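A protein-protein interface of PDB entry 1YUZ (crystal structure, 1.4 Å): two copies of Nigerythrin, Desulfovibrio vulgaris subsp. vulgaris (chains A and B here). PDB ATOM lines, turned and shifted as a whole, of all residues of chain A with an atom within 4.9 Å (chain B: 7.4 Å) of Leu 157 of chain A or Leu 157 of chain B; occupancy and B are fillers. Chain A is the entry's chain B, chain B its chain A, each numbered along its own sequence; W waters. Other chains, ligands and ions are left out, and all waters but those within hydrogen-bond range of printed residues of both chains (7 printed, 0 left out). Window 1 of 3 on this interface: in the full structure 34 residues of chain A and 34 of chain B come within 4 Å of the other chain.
Of chain B, only Ala 153 and Leu 157 come within 4 Å of Leu 157 of chain A.
Leu 157 of chain B touches just these residues of chain A: Ser 150, Ala 153 and Leu 157.
Of the printed residues of chain A, Asn 113 of chain B touches Ile 116 (3.5 Å).
Of the printed residues of chain A, Ala 158 of chain B touches Glu 154 (3.5 Å).
Ile 163 of chain B touches none of the printed residues of chain A.
Glu 115 of chain B touches none of the printed residues of chain A.
The nearest residue of chain A that does not touch Leu 157 of chain B is Glu 154 of chain A (4.1 Å).
The nearest printed residue of chain A that does not touch Ser 150 of chain B is Leu 157 of chain A (5.0 Å).
O of Ile 109 of chain B sits close to ND2 of Asn 113 of chain B, 3.4 Å away.
The backbone carbonyl oxygen (O) of Leu 157 of chain B is in hydrogen-bond range of the side-chain amide nitrogen (ND2) of Asn 161 of chain B (3.3 Å).
The backbone carbonyl oxygen of Leu 157 of chain A lies within hydrogen-bond range of the side-chain amide nitrogen of Asn 161 of chain A (3.3 Å).
Ile 109 of chain B touches Ile 116 of chain A (CG2 to CG2, 3.8 Å).
Ile 116 of chain A touches Asn 113 of chain B.
Ile 116 of chain B touches Ile 116 of chain A.
Ser 150 of chain A touches Tyr 160 of chain B (CB to CE2, 3.6 Å).
Leu 157 of chain A touches Ala 153 of chain B (CD1 to O, 3.7 Å).
Ala 158 of chain A touches Glu 154 of chain B (CA to OE2, 3.5 Å).
Of the 13 printed residues of chain A, 9 touch a printed residue of chain B.
Hydrophobic or aromatic side chains of chain A that line the printed part of chain B: Ile 109, Ile 116, Ala 153, Leu 157, Ala 158 and Tyr 160.
Printed residues of chain B that touch a printed residue of chain A: Asn 15, Ile 109, Asn 113, Ile 116, Thr 119, Ser 150, Val 151, Ala 153, Glu 154, Leu 157, Ala 158, Tyr 160 and Asn 161.
Among the printed residues, 19 pairs touch across the chains.
Among the printed residues, no Asp or Glu carboxylate lies within 4 Å of a Lys or Arg side-chain nitrogen of the other chain.
The backbone carbonyl oxygen of Tyr 160 of chain A sits at hydrogen-bond distance from the side-chain amide nitrogen of Asn 15 of chain B (2.9 Å).
The side-chain hydroxyl (OG) of Ser 150 of chain B lies within hydrogen-bond range of the side-chain amide oxygen (OD1) of Asn 161 of chain A, 2.6 Å away.
The side-chain amide nitrogen of Asn 161 of chain A sits at hydrogen-bond distance from the side-chain carboxylate of Glu 154 of chain B, 2.8 Å away.
The side-chain hydroxyl of Ser 150 of chain A is in hydrogen-bond range of the side-chain amide oxygen of Asn 161 of chain B (2.6 Å).
ND2 of Asn 161 of chain B is in hydrogen-bond range of OE2 of Glu 154 of chain A (2.8 Å).
Ala 153 of chain A touches Leu 157 of chain B, and with the chains exchanged Leu 157 of chain A touches Ala 153 of chain B.
Glu 154 of chain A touches Asn 161 of chain B, and with the chains exchanged Asn 161 of chain A touches Glu 154 of chain B.
Of the 19 pairs that touch across the chains among the printed residues, 14 have their exchanged pair printed and touching as well.
Water W5 bridges OE1 of Glu 154 of chain B (2.6 Å) and OE1 of Glu 154 of chain A (2.7 Å).
Water W2 lies within hydrogen-bond range of the side-chain hydroxyl (OG) of Ser 150 of chain B and the side-chain amide oxygen (OD1) of Asn 161 of chain A.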
ATOM      1  N   ILE A 109      26.290  12.363 -29.970  1.00  0.00           N
ATOM      2  CA  ILE A 109      26.231  13.752 -29.522  1.00  0.00           C
ATOM      3  C   ILE A 109      24.886  14.367 -29.928  1.00  0.00           C
ATOM      4  O   ILE A 109      24.261  15.081 -29.144  1.00  0.00           O
ATOM      5  CB  ILE A 109      27.398  14.583 -30.117  1.00  0.00           C
ATOM      6  CG1 ILE A 109      28.727  14.126 -29.500  1.00  0.00           C
ATOM      7  CG2 ILE A 109      27.161  16.071 -29.880  1.00  0.00           C
ATOM      8  CD1 ILE A 109      28.844  14.365 -27.994  1.00  0.00           C
ATOM      9  N   ALA A 112      22.411  13.006 -27.530  1.00  0.00           N
ATOM     10  CA  ALA A 112      22.542  13.632 -26.224  1.00  0.00           C
ATOM     11  C   ALA A 112      21.959  15.039 -26.222  1.00  0.00           C
ATOM     12  O   ALA A 112      21.249  15.417 -25.290  1.00  0.00           O
ATOM     13  CB  ALA A 112      24.001  13.669 -25.809  1.00  0.00           C
ATOM     14  N   ILE A 116      18.847  16.262 -23.965  1.00  0.00           N
ATOM     15  CA  ILE A 116      18.992  17.376 -23.040  1.00  0.00           C
ATOM     16  C   ILE A 116      17.918  18.430 -23.313  1.00  0.00           C
ATOM     17  O   ILE A 116      17.324  18.968 -22.381  1.00  0.00           O
ATOM     18  CB  ILE A 116      20.403  17.984 -23.154  1.00  0.00           C
ATOM     19  CG1 ILE A 116      21.424  17.002 -22.571  1.00  0.00           C
ATOM     20  CG2 ILE A 116      20.470  19.315 -22.428  1.00  0.00           C
ATOM     21  CD1 ILE A 116      22.870  17.383 -22.846  1.00  0.00           C
ATOM     22  N   SER A 150      16.626  12.427 -19.498  1.00  0.00           N
ATOM     23  CA  SER A 150      17.919  12.757 -18.925  1.00  0.00           C
ATOM     24  C   SER A 150      18.749  11.485 -18.734  1.00  0.00           C
ATOM     25  O   SER A 150      19.974  11.532 -18.770  1.00  0.00           O
ATOM     26  CB  SER A 150      17.754  13.532 -17.615  1.00  0.00           C
ATOM     27  OG  SER A 150      16.939  12.844 -16.691  1.00  0.00           O
ATOM     28  N   ALA A 153      20.224  10.826 -22.065  1.00  0.00           N
ATOM     29  CA  ALA A 153      21.342  11.728 -22.305  1.00  0.00           C
ATOM     30  C   ALA A 153      22.604  11.165 -21.661  1.00  0.00           C
ATOM     31  O   ALA A 153      23.664  11.131 -22.285  1.00  0.00           O
ATOM     32  CB  ALA A 153      21.035  13.113 -21.745  1.00  0.00           C
ATOM     33  N   GLU A 154      22.493  10.713 -20.414  1.00  0.00           N
ATOM     34  CA  GLU A 154      23.653  10.162 -19.729  1.00  0.00           C
ATOM     35  C   GLU A 154      24.158   8.900 -20.421  1.00  0.00           C
ATOM     36  O   GLU A 154      25.364   8.715 -20.569  1.00  0.00           O
ATOM     37  CB  GLU A 154      23.323   9.850 -18.269  1.00  0.00           C
ATOM     38  CG  GLU A 154      24.518   9.295 -17.513  1.00  0.00           C
ATOM     39  CD  GLU A 154      24.222   8.967 -16.066  1.00  0.00           C
ATOM     40  OE1 GLU A 154      25.097   8.360 -15.412  1.00  0.00           O
ATOM     41  OE2 GLU A 154      23.127   9.317 -15.574  1.00  0.00           O
ATOM     42  N   ARG A 155      23.242   8.037 -20.847  1.00  0.00           N
ATOM     43  CA  ARG A 155      23.630   6.803 -21.523  1.00  0.00           C
ATOM     44  C   ARG A 155      24.387   7.116 -22.811  1.00  0.00           C
ATOM     45  O   ARG A 155      25.373   6.460 -23.128  1.00  0.00           O
ATOM     46  CB  ARG A 155      22.389   5.958 -21.832  1.00  0.00           C
ATOM     47  CG  ARG A 155      21.742   5.324 -20.598  1.00  0.00           C
ATOM     48  CD  ARG A 155      22.204   3.883 -20.387  1.00  0.00           C
ATOM     49  NE  ARG A 155      23.654   3.744 -20.295  1.00  0.00           N
ATOM     50  CZ  ARG A 155      24.387   4.139 -19.258  1.00  0.00           C
ATOM     51  NH1 ARG A 155      23.805   4.705 -18.211  1.00  0.00           N
ATOM     52  NH2 ARG A 155      25.704   3.956 -19.268  1.00  0.00           N
ATOM     53  N   TYR A 156      23.933   8.121 -23.550  1.00  0.00           N
ATOM     54  CA  TYR A 156      24.600   8.491 -24.791  1.00  0.00           C
ATOM     55  C   TYR A 156      25.994   9.046 -24.524  1.00  0.00           C
ATOM     56  O   TYR A 156      26.936   8.737 -25.249  1.00  0.00           O
ATOM     57  CB  TYR A 156      23.764   9.518 -25.555  1.00  0.00           C
ATOM     58  CG  TYR A 156      22.562   8.935 -26.276  1.00  0.00           C
ATOM     59  CD1 TYR A 156      21.418   9.703 -26.488  1.00  0.00           C
ATOM     60  CD2 TYR A 156      22.593   7.643 -26.804  1.00  0.00           C
ATOM     61  CE1 TYR A 156      20.340   9.206 -27.213  1.00  0.00           C
ATOM     62  CE2 TYR A 156      21.521   7.135 -27.533  1.00  0.00           C
ATOM     63  CZ  TYR A 156      20.401   7.921 -27.735  1.00  0.00           C
ATOM     64  OH  TYR A 156      19.349   7.428 -28.479  1.00  0.00           O
ATOM     65  N   LEU A 157      26.134   9.865 -23.487  1.00  0.00           N
ATOM     66  CA  LEU A 157      27.441  10.426 -23.167  1.00  0.00           C
ATOM     67  C   LEU A 157      28.389   9.332 -22.680  1.00  0.00           C
ATOM     68  O   LEU A 157      29.574   9.341 -23.006  1.00  0.00           O
ATOM     69  CB  LEU A 157      27.302  11.534 -22.119  1.00  0.00           C
ATOM     70  CG  LEU A 157      26.507  12.755 -22.601  1.00  0.00           C
ATOM     71  CD1 LEU A 157      26.203  13.681 -21.439  1.00  0.00           C
ATOM     72  CD2 LEU A 157      27.291  13.490 -23.670  1.00  0.00           C
ATOM     73  N   ALA A 158      27.870   8.379 -21.911  1.00  0.00           N
ATOM     74  CA  ALA A 158      28.693   7.276 -21.420  1.00  0.00           C
ATOM     75  C   ALA A 158      29.186   6.461 -22.611  1.00  0.00           C
ATOM     76  O   ALA A 158      30.353   6.075 -22.677  1.00  0.00           O
ATOM     77  CB  ALA A 158      27.882   6.390 -20.482  1.00  0.00           C
ATOM     78  N   ALA A 159      28.292   6.203 -23.558  1.00  0.00           N
ATOM     79  CA  ALA A 159      28.645   5.432 -24.745  1.00  0.00           C
ATOM     80  C   ALA A 159      29.674   6.181 -25.583  1.00  0.00           C
ATOM     81  O   ALA A 159      30.560   5.575 -26.182  1.00  0.00           O
ATOM     82  CB  ALA A 159      27.401   5.156 -25.572  1.00  0.00           C
ATOM     83  N   TYR A 160      29.552   7.503 -25.624  1.00  0.00           N
ATOM     84  CA  TYR A 160      30.477   8.341 -26.379  1.00  0.00           C
ATOM     85  C   TYR A 160      31.864   8.274 -25.740  1.00  0.00           C
ATOM     86  O   TYR A 160      32.872   8.129 -26.431  1.00  0.00           O
ATOM     87  CB  TYR A 160      29.963   9.783 -26.379  1.00  0.00           C
ATOM     88  CG  TYR A 160      30.829  10.788 -27.110  1.00  0.00           C
ATOM     89  CD1 TYR A 160      30.642  11.047 -28.468  1.00  0.00           C
ATOM     90  CD2 TYR A 160      31.791  11.530 -26.425  1.00  0.00           C
ATOM     91  CE1 TYR A 160      31.382  12.029 -29.120  1.00  0.00           C
ATOM     92  CE2 TYR A 160      32.537  12.511 -27.068  1.00  0.00           C
ATOM     93  CZ  TYR A 160      32.322  12.756 -28.411  1.00  0.00           C
ATOM     94  OH  TYR A 160      33.026  13.757 -29.034  1.00  0.00           O
ATOM     95  N   ASN A 161      31.915   8.372 -24.416  1.00  0.00           N
ATOM     96  CA  ASN A 161      33.189   8.323 -23.711  1.00  0.00           C
ATOM     97  C   ASN A 161      33.874   6.974 -23.856  1.00  0.00           C
ATOM     98  O   ASN A 161      35.102   6.900 -23.884  1.00  0.00           O
ATOM     99  CB  ASN A 161      32.990   8.654 -22.234  1.00  0.00           C
ATOM    100  CG  ASN A 161      32.674  10.109 -22.019  1.00  0.00           C
ATOM    101  OD1 ASN A 161      33.108  10.951 -22.795  1.00  0.00           O
ATOM    102  ND2 ASN A 161      31.930  10.418 -20.972  1.00  0.00           N
ATOM    103  N   ASN B  15      36.037   9.093 -31.481  1.00  0.00           N
ATOM    104  CA  ASN B  15      35.093  10.132 -31.085  1.00  0.00           C
ATOM    105  C   ASN B  15      35.733  11.513 -31.199  1.00  0.00           C
ATOM    106  O   ASN B  15      35.503  12.397 -30.374  1.00  0.00           O
ATOM    107  CB  ASN B  15      34.538   9.885 -29.667  1.00  0.00           C
ATOM    108  CG  ASN B  15      35.618   9.780 -28.602  1.00  0.00           C
ATOM    109  OD1 ASN B  15      36.812   9.786 -28.893  1.00  0.00           O
ATOM    110  ND2 ASN B  15      35.189   9.677 -27.350  1.00  0.00           N
ATOM    111  N   LEU B  65      31.420  18.892  -7.146  1.00  0.00           N
ATOM    112  CA  LEU B  65      31.637  18.481  -8.529  1.00  0.00           C
ATOM    113  C   LEU B  65      31.973  19.717  -9.355  1.00  0.00           C
ATOM    114  O   LEU B  65      32.896  19.690 -10.169  1.00  0.00           O
ATOM    115  CB  LEU B  65      30.393  17.793  -9.100  1.00  0.00           C
ATOM    116  CG  LEU B  65      30.489  17.439 -10.591  1.00  0.00           C
ATOM    117  CD1 LEU B  65      31.686  16.537 -10.854  1.00  0.00           C
ATOM    118  CD2 LEU B  65      29.209  16.758 -11.023  1.00  0.00           C
ATOM    119  N   LEU B 108      23.710  22.508 -14.023  1.00  0.00           N
ATOM    120  CA  LEU B 108      24.298  21.241 -14.442  1.00  0.00           C
ATOM    121  C   LEU B 108      24.085  21.069 -15.941  1.00  0.00           C
ATOM    122  O   LEU B 108      24.979  20.618 -16.652  1.00  0.00           O
ATOM    123  CB  LEU B 108      23.659  20.070 -13.690  1.00  0.00           C
ATOM    124  CG  LEU B 108      24.103  19.907 -12.236  1.00  0.00           C
ATOM    125  CD1 LEU B 108      23.198  18.907 -11.534  1.00  0.00           C
ATOM    126  CD2 LEU B 108      25.553  19.448 -12.188  1.00  0.00           C
ATOM    127  N   ILE B 109      22.899  21.437 -16.421  1.00  0.00           N
ATOM    128  CA  ILE B 109      22.587  21.332 -17.842  1.00  0.00           C
ATOM    129  C   ILE B 109      23.443  22.315 -18.640  1.00  0.00           C
ATOM    130  O   ILE B 109      23.983  21.957 -19.685  1.00  0.00           O
ATOM    131  CB  ILE B 109      21.087  21.612 -18.108  1.00  0.00           C
ATOM    132  CG1 ILE B 109      20.238  20.484 -17.513  1.00  0.00           C
ATOM    133  CG2 ILE B 109      20.832  21.767 -19.606  1.00  0.00           C
ATOM    134  CD1 ILE B 109      20.413  19.131 -18.188  1.00  0.00           C
ATOM    135  N   GLY B 111      26.267  23.402 -17.819  1.00  0.00           N
ATOM    136  CA  GLY B 111      27.606  22.846 -17.798  1.00  0.00           C
ATOM    137  C   GLY B 111      27.725  21.744 -18.835  1.00  0.00           C
ATOM    138  O   GLY B 111      28.654  21.730 -19.639  1.00  0.00           O
ATOM    139  N   ALA B 112      26.771  20.820 -18.831  1.00  0.00           N
ATOM    140  CA  ALA B 112      26.790  19.720 -19.783  1.00  0.00           C
ATOM    141  C   ALA B 112      26.824  20.239 -21.215  1.00  0.00           C
ATOM    142  O   ALA B 112      27.593  19.746 -22.036  1.00  0.00           O
ATOM    143  CB  ALA B 112      25.578  18.831 -19.579  1.00  0.00           C
ATOM    144  N   ASN B 113      25.998  21.237 -21.521  1.00  0.00           N
ATOM    145  CA  ASN B 113      25.969  21.778 -22.873  1.00  0.00           C
ATOM    146  C   ASN B 113      27.302  22.395 -23.272  1.00  0.00           C
ATOM    147  O   ASN B 113      27.752  22.235 -24.409  1.00  0.00           O
ATOM    148  CB  ASN B 113      24.838  22.799 -23.022  1.00  0.00           C
ATOM    149  CG  ASN B 113      23.468  22.140 -23.041  1.00  0.00           C
ATOM    150  OD1 ASN B 113      23.332  20.992 -23.467  1.00  0.00           O
ATOM    151  ND2 ASN B 113      22.450  22.864 -22.591  1.00  0.00           N
ATOM    152  N   GLU B 115      30.261  21.585 -22.057  1.00  0.00           N
ATOM    153  CA  GLU B 115      31.215  20.488 -22.174  1.00  0.00           C
ATOM    154  C   GLU B 115      31.042  19.775 -23.505  1.00  0.00           C
ATOM    155  O   GLU B 115      32.020  19.398 -24.151  1.00  0.00           O
ATOM    156  CB  GLU B 115      31.010  19.479 -21.046  1.00  0.00           C
ATOM    157  CG  GLU B 115      31.268  20.018 -19.649  1.00  0.00           C
ATOM    158  CD  GLU B 115      32.725  20.376 -19.398  1.00  0.00           C
ATOM    159  OE1 GLU B 115      33.610  19.946 -20.168  1.00  0.00           O
ATOM    160  OE2 GLU B 115      32.993  21.076 -18.403  1.00  0.00           O
ATOM    161  N   ILE B 116      29.791  19.578 -23.907  1.00  0.00           N
ATOM    162  CA  ILE B 116      29.502  18.916 -25.166  1.00  0.00           C
ATOM    163  C   ILE B 116      30.030  19.766 -26.314  1.00  0.00           C
ATOM    164  O   ILE B 116      30.626  19.244 -27.251  1.00  0.00           O
ATOM    165  CB  ILE B 116      27.990  18.664 -25.310  1.00  0.00           C
ATOM    166  CG1 ILE B 116      27.574  17.563 -24.325  1.00  0.00           C
ATOM    167  CG2 ILE B 116      27.648  18.268 -26.743  1.00  0.00           C
ATOM    168  CD1 ILE B 116      26.078  17.402 -24.157  1.00  0.00           C
ATOM    169  N   THR B 119      33.872  19.328 -26.353  1.00  0.00           N
ATOM    170  CA  THR B 119      34.353  18.017 -26.755  1.00  0.00           C
ATOM    171  C   THR B 119      34.013  17.612 -28.184  1.00  0.00           C
ATOM    172  O   THR B 119      34.748  16.838 -28.789  1.00  0.00           O
ATOM    173  CB  THR B 119      33.833  16.904 -25.806  1.00  0.00           C
ATOM    174  OG1 THR B 119      34.714  15.776 -25.879  1.00  0.00           O
ATOM    175  CG2 THR B 119      32.430  16.446 -26.214  1.00  0.00           C
ATOM    176  N   GLU B 149      36.577  16.823 -21.324  1.00  0.00           N
ATOM    177  CA  GLU B 149      35.298  17.509 -21.451  1.00  0.00           C
ATOM    178  C   GLU B 149      34.109  16.567 -21.584  1.00  0.00           C
ATOM    179  O   GLU B 149      33.054  16.817 -21.000  1.00  0.00           O
ATOM    180  CB  GLU B 149      35.328  18.479 -22.635  1.00  0.00           C
ATOM    181  CG  GLU B 149      36.562  19.389 -22.673  1.00  0.00           C
ATOM    182  CD  GLU B 149      36.702  20.303 -21.462  1.00  0.00           C
ATOM    183  OE1 GLU B 149      36.530  19.835 -20.316  1.00  0.00           O
ATOM    184  OE2 GLU B 149      37.007  21.498 -21.658  1.00  0.00           O
ATOM    185  N   SER B 150      34.258  15.487 -22.341  1.00  0.00           N
ATOM    186  CA  SER B 150      33.139  14.566 -22.472  1.00  0.00           C
ATOM    187  C   SER B 150      32.915  13.826 -21.152  1.00  0.00           C
ATOM    188  O   SER B 150      31.788  13.453 -20.836  1.00  0.00           O
ATOM    189  CB  SER B 150      33.357  13.600 -23.643  1.00  0.00           C
ATOM    190  OG  SER B 150      34.595  12.932 -23.550  1.00  0.00           O
ATOM    191  N   VAL B 151      33.979  13.627 -20.376  1.00  0.00           N
ATOM    192  CA  VAL B 151      33.845  12.990 -19.070  1.00  0.00           C
ATOM    193  C   VAL B 151      33.075  13.968 -18.174  1.00  0.00           C
ATOM    194  O   VAL B 151      32.191  13.565 -17.422  1.00  0.00           O
ATOM    195  CB  VAL B 151      35.227  12.683 -18.439  1.00  0.00           C
ATOM    196  CG1 VAL B 151      35.069  12.331 -16.963  1.00  0.00           C
ATOM    197  CG2 VAL B 151      35.885  11.525 -19.177  1.00  0.00           C
ATOM    198  N   HIS B 152      33.405  15.254 -18.258  1.00  0.00           N
ATOM    199  CA  HIS B 152      32.710  16.264 -17.465  1.00  0.00           C
ATOM    200  C   HIS B 152      31.226  16.288 -17.819  1.00  0.00           C
ATOM    201  O   HIS B 152      30.372  16.411 -16.940  1.00  0.00           O
ATOM    202  CB  HIS B 152      33.296  17.649 -17.722  1.00  0.00           C
ATOM    203  CG  HIS B 152      34.724  17.791 -17.298  1.00  0.00           C
ATOM    204  ND1 HIS B 152      35.500  18.867 -17.670  1.00  0.00           N
ATOM    205  CD2 HIS B 152      35.520  16.994 -16.546  1.00  0.00           C
ATOM    206  CE1 HIS B 152      36.713  18.725 -17.168  1.00  0.00           C
ATOM    207  NE2 HIS B 152      36.752  17.597 -16.482  1.00  0.00           N
ATOM    208  N   ALA B 153      30.916  16.176 -19.108  1.00  0.00           N
ATOM    209  CA  ALA B 153      29.527  16.183 -19.544  1.00  0.00           C
ATOM    210  C   ALA B 153      28.771  15.032 -18.897  1.00  0.00           C
ATOM    211  O   ALA B 153      27.664  15.217 -18.392  1.00  0.00           O
ATOM    212  CB  ALA B 153      29.449  16.069 -21.060  1.00  0.00           C
ATOM    213  N   GLU B 154      29.368  13.845 -18.912  1.00  0.00           N
ATOM    214  CA  GLU B 154      28.723  12.687 -18.321  1.00  0.00           C
ATOM    215  C   GLU B 154      28.550  12.876 -16.820  1.00  0.00           C
ATOM    216  O   GLU B 154      27.506  12.540 -16.272  1.00  0.00           O
ATOM    217  CB  GLU B 154      29.528  11.417 -18.604  1.00  0.00           C
ATOM    218  CG  GLU B 154      28.852  10.165 -18.059  1.00  0.00           C
ATOM    219  CD  GLU B 154      29.656   8.899 -18.273  1.00  0.00           C
ATOM    220  OE1 GLU B 154      29.305   7.875 -17.653  1.00  0.00           O
ATOM    221  OE2 GLU B 154      30.626   8.919 -19.062  1.00  0.00           O
ATOM    222  N   ARG B 155      29.568  13.413 -16.153  1.00  0.00           N
ATOM    223  CA  ARG B 155      29.476  13.644 -14.714  1.00  0.00           C
ATOM    224  C   ARG B 155      28.341  14.609 -14.389  1.00  0.00           C
ATOM    225  O   ARG B 155      27.618  14.414 -13.414  1.00  0.00           O
ATOM    226  CB  ARG B 155      30.796  14.197 -14.174  1.00  0.00           C
ATOM    227  CG  ARG B 155      31.926  13.172 -14.137  1.00  0.00           C
ATOM    228  CD  ARG B 155      32.079  12.539 -12.756  1.00  0.00           C
ATOM    229  NE  ARG B 155      30.853  11.915 -12.265  1.00  0.00           N
ATOM    230  CZ  ARG B 155      30.378  10.751 -12.695  1.00  0.00           C
ATOM    231  NH1 ARG B 155      31.027  10.072 -13.631  1.00  0.00           N
ATOM    232  NH2 ARG B 155      29.250  10.266 -12.187  1.00  0.00           N
ATOM    233  N   TYR B 156      28.171  15.646 -15.206  1.00  0.00           N
ATOM    234  CA  TYR B 156      27.107  16.611 -14.969  1.00  0.00           C
ATOM    235  C   TYR B 156      25.732  15.982 -15.175  1.00  0.00           C
ATOM    236  O   TYR B 156      24.809  16.240 -14.407  1.00  0.00           O
ATOM    237  CB  TYR B 156      27.283  17.827 -15.885  1.00  0.00           C
ATOM    238  CG  TYR B 156      28.354  18.798 -15.426  1.00  0.00           C
ATOM    239  CD1 TYR B 156      29.044  19.584 -16.346  1.00  0.00           C
ATOM    240  CD2 TYR B 156      28.638  18.969 -14.072  1.00  0.00           C
ATOM    241  CE1 TYR B 156      29.984  20.518 -15.929  1.00  0.00           C
ATOM    242  CE2 TYR B 156      29.574  19.900 -13.644  1.00  0.00           C
ATOM    243  CZ  TYR B 156      30.242  20.673 -14.575  1.00  0.00           C
ATOM    244  OH  TYR B 156      31.153  21.610 -14.139  1.00  0.00           O
ATOM    245  N   LEU B 157      25.583  15.156 -16.205  1.00  0.00           N
ATOM    246  CA  LEU B 157      24.293  14.508 -16.433  1.00  0.00           C
ATOM    247  C   LEU B 157      23.999  13.498 -15.330  1.00  0.00           C
ATOM    248  O   LEU B 157      22.854  13.363 -14.903  1.00  0.00           O
ATOM    249  CB  LEU B 157      24.254  13.813 -17.796  1.00  0.00           C
ATOM    250  CG  LEU B 157      23.455  14.528 -18.893  1.00  0.00           C
ATOM    251  CD1 LEU B 157      22.001  14.665 -18.470  1.00  0.00           C
ATOM    252  CD2 LEU B 157      24.053  15.891 -19.164  1.00  0.00           C
ATOM    253  N   ALA B 158      25.023  12.789 -14.865  1.00  0.00           N
ATOM    254  CA  ALA B 158      24.832  11.816 -13.793  1.00  0.00           C
ATOM    255  C   ALA B 158      24.361  12.548 -12.539  1.00  0.00           C
ATOM    256  O   ALA B 158      23.458  12.088 -11.845  1.00  0.00           O
ATOM    257  CB  ALA B 158      26.131  11.080 -13.512  1.00  0.00           C
ATOM    258  N   ALA B 159      24.975  13.692 -12.253  1.00  0.00           N
ATOM    259  CA  ALA B 159      24.606  14.483 -11.083  1.00  0.00           C
ATOM    260  C   ALA B 159      23.177  15.004 -11.228  1.00  0.00           C
ATOM    261  O   ALA B 159      22.417  15.049 -10.262  1.00  0.00           O
ATOM    262  CB  ALA B 159      25.576  15.643 -10.912  1.00  0.00           C
ATOM    263  N   TYR B 160      22.814  15.398 -12.443  1.00  0.00           N
ATOM    264  CA  TYR B 160      21.474  15.900 -12.729  1.00  0.00           C
ATOM    265  C   TYR B 160      20.445  14.795 -12.478  1.00  0.00           C
ATOM    266  O   TYR B 160      19.422  15.022 -11.833  1.00  0.00           O
ATOM    267  CB  TYR B 160      21.412  16.360 -14.189  1.00  0.00           C
ATOM    268  CG  TYR B 160      20.092  16.939 -14.651  1.00  0.00           C
ATOM    269  CD1 TYR B 160      19.831  18.309 -14.554  1.00  0.00           C
ATOM    270  CD2 TYR B 160      19.137  16.131 -15.261  1.00  0.00           C
ATOM    271  CE1 TYR B 160      18.657  18.857 -15.065  1.00  0.00           C
ATOM    272  CE2 TYR B 160      17.963  16.665 -15.776  1.00  0.00           C
ATOM    273  CZ  TYR B 160      17.728  18.029 -15.679  1.00  0.00           C
ATOM    274  OH  TYR B 160      16.581  18.543 -16.237  1.00  0.00           O
ATOM    275  N   ASN B 161      20.719  13.595 -12.975  1.00  0.00           N
ATOM    276  CA  ASN B 161      19.786  12.493 -12.790  1.00  0.00           C
ATOM    277  C   ASN B 161      19.613  12.092 -11.333  1.00  0.00           C
ATOM    278  O   ASN B 161      18.540  11.629 -10.942  1.00  0.00           O
ATOM    279  CB  ASN B 161      20.215  11.287 -13.629  1.00  0.00           C
ATOM    280  CG  ASN B 161      20.057  11.539 -15.110  1.00  0.00           C
ATOM    281  OD1 ASN B 161      19.197  12.313 -15.521  1.00  0.00           O
ATOM    282  ND2 ASN B 161      20.875  10.886 -15.921  1.00  0.00           N
ATOM    283  N   ASP B 162      20.656  12.284 -10.530  1.00  0.00           N
ATOM    284  CA  ASP B 162      20.596  11.943  -9.112  1.00  0.00           C
ATOM    285  C   ASP B 162      20.649  13.187  -8.242  1.00  0.00           C
ATOM    286  O   ASP B 162      21.149  13.144  -7.123  1.00  0.00           O
ATOM    287  CB  ASP B 162      21.756  11.021  -8.726  1.00  0.00           C
ATOM    288  CG  ASP B 162      21.560   9.608  -9.212  1.00  0.00           C
ATOM    289  OD1 ASP B 162      20.397   9.160  -9.262  1.00  0.00           O
ATOM    290  OD2 ASP B 162      22.568   8.939  -9.527  1.00  0.00           O
ATOM    291  N   ILE B 163      20.112  14.291  -8.746  1.00  0.00           N
ATOM    292  CA  ILE B 163      20.152  15.542  -8.003  1.00  0.00           C
ATOM    293  C   ILE B 163      19.545  15.443  -6.607  1.00  0.00           C
ATOM    294  O   ILE B 163      19.980  16.135  -5.690  1.00  0.00           O
ATOM    295  CB  ILE B 163      19.460  16.676  -8.793  1.00  0.00           C
ATOM    296  CG1 ILE B 163      19.730  18.015  -8.110  1.00  0.00           C
ATOM    297  CG2 ILE B 163      17.968  16.413  -8.902  1.00  0.00           C
ATOM    298  CD1 ILE B 163      19.374  19.217  -8.959  1.00  0.00           C
HETATM  299  O   HOH W   1      31.830   6.350 -19.893  1.00  0.00           O
HETATM  300  O   HOH W   2      36.582  10.922 -22.783  1.00  0.00           O
HETATM  301  O   HOH W   3      36.620   9.100 -24.810  1.00  0.00           O
HETATM  302  O   HOH W   4      21.603   8.563 -13.735  1.00  0.00           O
HETATM  303  O   HOH W   5      27.220   7.011 -16.314  1.00  0.00           O
HETATM  304  O   HOH W   6      33.094   9.070 -18.102  1.00  0.00           O
HETATM  305  O   HOH W   7      32.663  13.821 -31.664  1.00  0.00           O
